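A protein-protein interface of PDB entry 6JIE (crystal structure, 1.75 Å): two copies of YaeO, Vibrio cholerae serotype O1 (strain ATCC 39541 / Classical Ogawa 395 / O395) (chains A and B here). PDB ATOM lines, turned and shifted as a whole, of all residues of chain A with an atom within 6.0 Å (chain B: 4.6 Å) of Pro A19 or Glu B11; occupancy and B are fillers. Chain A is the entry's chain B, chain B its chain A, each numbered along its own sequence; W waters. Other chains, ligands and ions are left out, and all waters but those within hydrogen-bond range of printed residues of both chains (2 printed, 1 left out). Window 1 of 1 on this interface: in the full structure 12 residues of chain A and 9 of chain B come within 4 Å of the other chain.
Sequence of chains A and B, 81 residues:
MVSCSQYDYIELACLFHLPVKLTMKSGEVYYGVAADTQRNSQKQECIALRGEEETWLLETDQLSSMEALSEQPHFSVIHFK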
ATOM      1  N   PHE A  16     -12.540   3.883  23.751  1.00  0.00           N
ATOM      2  CA  PHE A  16     -11.457   4.399  22.925  1.00  0.00           C
ATOM      3  C   PHE A  16     -10.183   4.693  23.718  1.00  0.00           C
ATOM      4  O   PHE A  16      -9.234   5.244  23.155  1.00  0.00           O
ATOM      5  CB  PHE A  16     -11.925   5.671  22.208  1.00  0.00           C
ATOM      6  CG  PHE A  16     -13.104   5.447  21.272  1.00  0.00           C
ATOM      7  CD1 PHE A  16     -13.093   4.402  20.363  1.00  0.00           C
ATOM      8  CD2 PHE A  16     -14.208   6.276  21.314  1.00  0.00           C
ATOM      9  CE1 PHE A  16     -14.164   4.192  19.482  1.00  0.00           C
ATOM     10  CE2 PHE A  16     -15.292   6.064  20.437  1.00  0.00           C
ATOM     11  CZ  PHE A  16     -15.259   5.015  19.536  1.00  0.00           C
ATOM     12  N   HIS A  17     -10.141   4.354  25.004  1.00  0.00           N
ATOM     13  CA  HIS A  17      -8.995   4.640  25.877  1.00  0.00           C
ATOM     14  C   HIS A  17      -8.547   6.090  25.748  1.00  0.00           C
ATOM     15  O   HIS A  17      -7.386   6.394  25.462  1.00  0.00           O
ATOM     16  CB  HIS A  17      -7.835   3.686  25.599  1.00  0.00           C
ATOM     17  CG  HIS A  17      -8.154   2.269  25.946  1.00  0.00           C
ATOM     18  ND1 HIS A  17      -8.729   1.920  27.147  1.00  0.00           N
ATOM     19  CD2 HIS A  17      -8.011   1.118  25.248  1.00  0.00           C
ATOM     20  CE1 HIS A  17      -8.902   0.612  27.187  1.00  0.00           C
ATOM     21  NE2 HIS A  17      -8.474   0.101  26.047  1.00  0.00           N
ATOM     22  N   LEU A  18      -9.484   6.974  25.974  1.00  0.00           N
ATOM     23  CA  LEU A  18      -9.192   8.383  25.768  1.00  0.00           C
ATOM     24  C   LEU A  18      -8.409   8.949  26.946  1.00  0.00           C
ATOM     25  O   LEU A  18      -8.696   8.611  28.093  1.00  0.00           O
ATOM     26  CB  LEU A  18     -10.483   9.172  25.605  1.00  0.00           C
ATOM     27  CG  LEU A  18     -11.313   8.869  24.357  1.00  0.00           C
ATOM     28  CD1 LEU A  18     -12.491   9.835  24.285  1.00  0.00           C
ATOM     29  CD2 LEU A  18     -10.455   8.977  23.105  1.00  0.00           C
ATOM     30  N   PRO A  19      -7.454   9.849  26.690  1.00  0.00           N
ATOM     31  CA  PRO A  19      -6.836  10.599  27.788  1.00  0.00           C
ATOM     32  C   PRO A  19      -7.826  11.613  28.337  1.00  0.00           C
ATOM     33  O   PRO A  19      -8.394  12.403  27.579  1.00  0.00           O
ATOM     34  CB  PRO A  19      -5.642  11.285  27.120  1.00  0.00           C
ATOM     35  CG  PRO A  19      -6.066  11.448  25.683  1.00  0.00           C
ATOM     36  CD  PRO A  19      -6.905  10.224  25.379  1.00  0.00           C
ATOM     37  N   VAL A  20      -8.039  11.584  29.657  1.00  0.00           N
ATOM     38  CA  VAL A  20      -9.042  12.438  30.285  1.00  0.00           C
ATOM     39  C   VAL A  20      -8.539  12.988  31.608  1.00  0.00           C
ATOM     40  O   VAL A  20      -7.694  12.391  32.277  1.00  0.00           O
ATOM     41  CB  VAL A  20     -10.386  11.718  30.531  1.00  0.00           C
ATOM     42  CG1 VAL A  20     -11.044  11.348  29.190  1.00  0.00           C
ATOM     43  CG2 VAL A  20     -10.211  10.490  31.394  1.00  0.00           C
ATOM     44  N   LYS A  21      -9.083  14.147  31.963  1.00  0.00           N
ATOM     45  CA  LYS A  21      -8.939  14.765  33.273  1.00  0.00           C
ATOM     46  C   LYS A  21     -10.274  14.623  33.990  1.00  0.00           C
ATOM     47  O   LYS A  21     -11.305  15.119  33.508  1.00  0.00           O
ATOM     48  CB  LYS A  21      -8.538  16.235  33.139  1.00  0.00           C
ATOM     49  CG  LYS A  21      -8.609  17.033  34.445  1.00  0.00           C
ATOM     50  CD  LYS A  21      -8.420  18.518  34.136  1.00  0.00           C
ATOM     51  CE  LYS A  21      -8.805  19.417  35.292  1.00  0.00           C
ATOM     52  NZ  LYS A  21      -8.897  20.844  34.834  1.00  0.00           N
ATOM     53  N   GLY A  32      -5.378  10.884  33.355  1.00  0.00           N
ATOM     54  CA  GLY A  32      -4.808   9.640  32.867  1.00  0.00           C
ATOM     55  C   GLY A  32      -5.568   9.130  31.663  1.00  0.00           C
ATOM     56  O   GLY A  32      -6.250   9.892  30.984  1.00  0.00           O
ATOM     57  N   VAL A  33      -5.450   7.825  31.432  1.00  0.00           N
ATOM     58  CA  VAL A  33      -6.108   7.155  30.322  1.00  0.00           C
ATOM     59  C   VAL A  33      -7.307   6.388  30.861  1.00  0.00           C
ATOM     60  O   VAL A  33      -7.178   5.598  31.810  1.00  0.00           O
ATOM     61  CB  VAL A  33      -5.132   6.224  29.586  1.00  0.00           C
ATOM     62  CG1 VAL A  33      -5.849   5.481  28.443  1.00  0.00           C
ATOM     63  CG2 VAL A  33      -3.939   7.034  29.080  1.00  0.00           C
ATOM     64  N   ALA A  34      -8.473   6.631  30.272  1.00  0.00           N
ATOM     65  CA  ALA A  34      -9.686   5.918  30.660  1.00  0.00           C
ATOM     66  C   ALA A  34      -9.571   4.455  30.260  1.00  0.00           C
ATOM     67  O   ALA A  34      -9.506   4.139  29.069  1.00  0.00           O
ATOM     68  CB  ALA A  34     -10.902   6.553  29.993  1.00  0.00           C
ATOM     69  N   GLU A  67     -12.898  15.848  31.320  1.00  0.00           N
ATOM     70  CA  GLU A  67     -12.355  16.740  30.301  1.00  0.00           C
ATOM     71  C   GLU A  67     -11.440  15.955  29.369  1.00  0.00           C
ATOM     72  O   GLU A  67     -10.564  15.219  29.826  1.00  0.00           O
ATOM     73  CB  GLU A  67     -11.584  17.895  30.955  1.00  0.00           C
ATOM     74  CG  GLU A  67     -10.833  18.798  29.985  1.00  0.00           C
ATOM     75  CD  GLU A  67     -10.188  19.975  30.676  1.00  0.00           C
ATOM     76  OE1 GLU A  67     -10.513  20.224  31.845  1.00  0.00           O
ATOM     77  OE2 GLU A  67      -9.374  20.671  30.046  1.00  0.00           O
ATOM     78  N   ALA A  68     -11.649  16.108  28.061  1.00  0.00           N
ATOM     79  CA  ALA A  68     -10.756  15.501  27.082  1.00  0.00           C
ATOM     80  C   ALA A  68      -9.366  16.124  27.139  1.00  0.00           C
ATOM     81  O   ALA A  68      -9.224  17.352  27.171  1.00  0.00           O
ATOM     82  CB  ALA A  68     -11.335  15.665  25.680  1.00  0.00           C
ATOM     83  N   LEU A  69      -8.331  15.280  27.133  1.00  0.00           N
ATOM     84  CA  LEU A  69      -6.958  15.751  27.010  1.00  0.00           C
ATOM     85  C   LEU A  69      -6.393  15.534  25.608  1.00  0.00           C
ATOM     86  O   LEU A  69      -5.189  15.709  25.395  1.00  0.00           O
ATOM     87  CB  LEU A  69      -6.054  15.076  28.048  1.00  0.00           C
ATOM     88  CG  LEU A  69      -6.444  15.350  29.501  1.00  0.00           C
ATOM     89  CD1 LEU A  69      -5.526  14.609  30.459  1.00  0.00           C
ATOM     90  CD2 LEU A  69      -6.449  16.854  29.787  1.00  0.00           C
ATOM     91  N   SER A  70      -7.228  15.160  24.653  1.00  0.00           N
ATOM     92  CA  SER A  70      -6.806  15.077  23.264  1.00  0.00           C
ATOM     93  C   SER A  70      -7.909  15.625  22.382  1.00  0.00           C
ATOM     94  O   SER A  70      -9.059  15.782  22.809  1.00  0.00           O
ATOM     95  CB  SER A  70      -6.492  13.635  22.844  1.00  0.00           C
ATOM     96  OG  SER A  70      -7.654  12.835  22.993  1.00  0.00           O
ATOM     97  N   GLN A  72     -10.584  15.068  19.861  1.00  0.00           N
ATOM     98  CA  GLN A  72     -11.454  14.029  19.336  1.00  0.00           C
ATOM     99  C   GLN A  72     -12.857  14.606  19.217  1.00  0.00           C
ATOM    100  O   GLN A  72     -13.157  15.642  19.821  1.00  0.00           O
ATOM    101  CB  GLN A  72     -11.429  12.769  20.222  1.00  0.00           C
ATOM    102  CG  GLN A  72     -11.191  13.001  21.700  1.00  0.00           C
ATOM    103  CD  GLN A  72     -12.478  13.267  22.450  1.00  0.00           C
ATOM    104  OE1 GLN A  72     -13.546  13.386  21.852  1.00  0.00           O
ATOM    105  NE2 GLN A  72     -12.379  13.360  23.764  1.00  0.00           N
ATOM    106  N   PHE A  75     -16.170  14.804  22.899  1.00  0.00           N
ATOM    107  CA  PHE A  75     -16.427  15.787  23.940  1.00  0.00           C
ATOM    108  C   PHE A  75     -15.181  16.626  24.182  1.00  0.00           C
ATOM    109  O   PHE A  75     -14.053  16.216  23.884  1.00  0.00           O
ATOM    110  CB  PHE A  75     -16.887  15.128  25.256  1.00  0.00           C
ATOM    111  CG  PHE A  75     -15.925  14.109  25.805  1.00  0.00           C
ATOM    112  CD1 PHE A  75     -14.901  14.491  26.663  1.00  0.00           C
ATOM    113  CD2 PHE A  75     -16.065  12.764  25.491  1.00  0.00           C
ATOM    114  CE1 PHE A  75     -14.028  13.551  27.179  1.00  0.00           C
ATOM    115  CE2 PHE A  75     -15.199  11.821  25.996  1.00  0.00           C
ATOM    116  CZ  PHE A  75     -14.176  12.215  26.852  1.00  0.00           C
ATOM    117  N   ASP B   8      -3.049   3.797  22.596  1.00  0.00           N
ATOM    118  CA  ASP B   8      -2.083   4.585  21.826  1.00  0.00           C
ATOM    119  C   ASP B   8      -0.913   4.901  22.746  1.00  0.00           C
ATOM    120  O   ASP B   8      -0.960   5.860  23.525  1.00  0.00           O
ATOM    121  CB  ASP B   8      -2.726   5.854  21.279  1.00  0.00           C
ATOM    122  CG  ASP B   8      -1.871   6.542  20.231  1.00  0.00           C
ATOM    123  OD1 ASP B   8      -0.650   6.266  20.180  1.00  0.00           O
ATOM    124  OD2 ASP B   8      -2.427   7.360  19.460  1.00  0.00           O
ATOM    125  N   TYR B   9       0.149   4.100  22.663  1.00  0.00           N
ATOM    126  CA  TYR B   9       1.261   4.302  23.587  1.00  0.00           C
ATOM    127  C   TYR B   9       2.094   5.520  23.235  1.00  0.00           C
ATOM    128  O   TYR B   9       2.755   6.070  24.116  1.00  0.00           O
ATOM    129  CB  TYR B   9       2.125   3.044  23.660  1.00  0.00           C
ATOM    130  CG  TYR B   9       1.431   2.000  24.508  1.00  0.00           C
ATOM    131  CD1 TYR B   9       1.347   2.149  25.891  1.00  0.00           C
ATOM    132  CD2 TYR B   9       0.804   0.910  23.927  1.00  0.00           C
ATOM    133  CE1 TYR B   9       0.673   1.216  26.682  1.00  0.00           C
ATOM    134  CE2 TYR B   9       0.148  -0.030  24.699  1.00  0.00           C
ATOM    135  CZ  TYR B   9       0.078   0.130  26.074  1.00  0.00           C
ATOM    136  OH  TYR B   9      -0.580  -0.795  26.834  1.00  0.00           O
ATOM    137  N   ILE B  10       2.076   5.957  21.979  1.00  0.00           N
ATOM    138  CA  ILE B  10       2.733   7.215  21.638  1.00  0.00           C
ATOM    139  C   ILE B  10       2.010   8.371  22.306  1.00  0.00           C
ATOM    140  O   ILE B  10       2.635   9.226  22.941  1.00  0.00           O
ATOM    141  CB  ILE B  10       2.795   7.396  20.114  1.00  0.00           C
ATOM    142  CG1 ILE B  10       3.604   6.268  19.496  1.00  0.00           C
ATOM    143  CG2 ILE B  10       3.423   8.738  19.766  1.00  0.00           C
ATOM    144  CD1 ILE B  10       3.652   6.339  17.992  1.00  0.00           C
ATOM    145  N   GLU B  11       0.674   8.377  22.212  1.00  0.00           N
ATOM    146  CA  GLU B  11      -0.136   9.402  22.855  1.00  0.00           C
ATOM    147  C   GLU B  11       0.083   9.395  24.363  1.00  0.00           C
ATOM    148  O   GLU B  11       0.276  10.448  24.977  1.00  0.00           O
ATOM    149  CB  GLU B  11      -1.608   9.172  22.510  1.00  0.00           C
ATOM    150  CG  GLU B  11      -2.604  10.146  23.107  1.00  0.00           C
ATOM    151  CD  GLU B  11      -4.019   9.756  22.764  1.00  0.00           C
ATOM    152  OE1 GLU B  11      -4.499   8.729  23.295  1.00  0.00           O
ATOM    153  OE2 GLU B  11      -4.643  10.454  21.934  1.00  0.00           O
ATOM    154  N   LEU B  12       0.069   8.203  24.966  1.00  0.00           N
ATOM    155  CA  LEU B  12       0.249   8.058  26.405  1.00  0.00           C
ATOM    156  C   LEU B  12       1.634   8.523  26.853  1.00  0.00           C
ATOM    157  O   LEU B  12       1.776   9.156  27.907  1.00  0.00           O
ATOM    158  CB  LEU B  12       0.005   6.595  26.784  1.00  0.00           C
ATOM    159  CG  LEU B  12       0.218   6.116  28.215  1.00  0.00           C
ATOM    160  CD1 LEU B  12      -0.706   4.950  28.482  1.00  0.00           C
ATOM    161  CD2 LEU B  12       1.648   5.686  28.418  1.00  0.00           C
ATOM    162  N   ALA B  13       2.673   8.197  26.084  1.00  0.00           N
ATOM    163  CA  ALA B  13       4.012   8.652  26.430  1.00  0.00           C
ATOM    164  C   ALA B  13       4.085  10.173  26.449  1.00  0.00           C
ATOM    165  O   ALA B  13       4.724  10.764  27.328  1.00  0.00           O
ATOM    166  CB  ALA B  13       5.037   8.082  25.442  1.00  0.00           C
ATOM    167  N   CYS B  14       3.440  10.823  25.482  1.00  0.00           N
ATOM    168  CA  CYS B  14       3.442  12.280  25.437  1.00  0.00           C
ATOM    169  C   CYS B  14       2.601  12.867  26.565  1.00  0.00           C
ATOM    170  O   CYS B  14       2.987  13.875  27.169  1.00  0.00           O
ATOM    171  CB  CYS B  14       2.948  12.759  24.073  1.00  0.00           C
ATOM    172  SG  CYS B  14       4.040  12.319  22.704  1.00  0.00           S
ATOM    173  N   LEU B  15       1.454  12.234  26.868  1.00  0.00           N
ATOM    174  CA  LEU B  15       0.567  12.681  27.940  1.00  0.00           C
ATOM    175  C   LEU B  15       1.307  12.811  29.261  1.00  0.00           C
ATOM    176  O   LEU B  15       1.114  13.782  30.001  1.00  0.00           O
ATOM    177  CB  LEU B  15      -0.591  11.690  28.102  1.00  0.00           C
ATOM    178  CG  LEU B  15      -1.547  11.903  29.273  1.00  0.00           C
ATOM    179  CD1 LEU B  15      -2.219  13.247  29.128  1.00  0.00           C
ATOM    180  CD2 LEU B  15      -2.570  10.774  29.354  1.00  0.00           C
HETATM  181  O   HOH W   1      -4.884   5.509  24.756  1.00  0.00           O
HETATM  182  O   HOH W   2      -7.085  10.644  21.665  1.00  0.00           O
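The backbone NH (N) of Glu B11 sits at hydrogen-bond distance from the side-chain carboxylate (OD1) of Asp B8, 3.2 Å away.
N of Leu A69 lies within hydrogen-bond range of O of Pro A19, at 2.9 Å.
Among the printed residues, pairs that only touch across the chains: Pro A19 with Glu B11 (3.5 Å), Pro A19 with Leu B15 (3.8 Å), Val A33 with Leu B12 (3.9 Å), Val A33 with Leu B15 (3.99 Å), Leu A69 with Leu B15 (3.8 Å) and Ser A70 with Glu B11 (3.8 Å).
Glu B11 touches just these residues of chain A: Pro A19 (3.5 Å) and Ser A70 (3.8 Å).
Of the printed residues of chain A, Leu B12 touches Val A33.
Of the printed residues of chain B, Ser A70 touches Glu B11.
Of the printed residues of chain A, Leu B15 touches Pro A19 (3.8 Å), Val A33 (3.99 Å) and Leu A69 (3.8 Å).
Of the printed residues of chain B, Leu A69 touches Leu B15 (3.8 Å).
Of the printed residues of chain B, Val A33 touches Leu B12 and Leu B15.
The nearest printed residue of chain B that does not touch Pro A19 is Leu B12 (6.8 Å).
Hydrophobic or aromatic side chains of chain B within 4 Å of the printed part of chain A: Leu B12 and Leu B15.
Along chain B the printed residues that touch a printed residue of chain A span positions 11 to 15.
Hydrophobic or aromatic side chains of chain A within 4 Å of the printed part of chain B: Pro A19, Val A33 and Leu A69.
Among the printed residues, no Asp or Glu carboxylate lies within 4 Å of a Lys or Arg side-chain nitrogen of the other chain.
No position is printed for both chains.
Water W2 lies within hydrogen-bond range of OE2 of Glu B11 and OG of Ser A70.
Water W1 lies within hydrogen-bond range of the backbone carbonyl oxygen of His A17 (2.7 Å) and the backbone NH of Asp B8 (3.3 Å).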
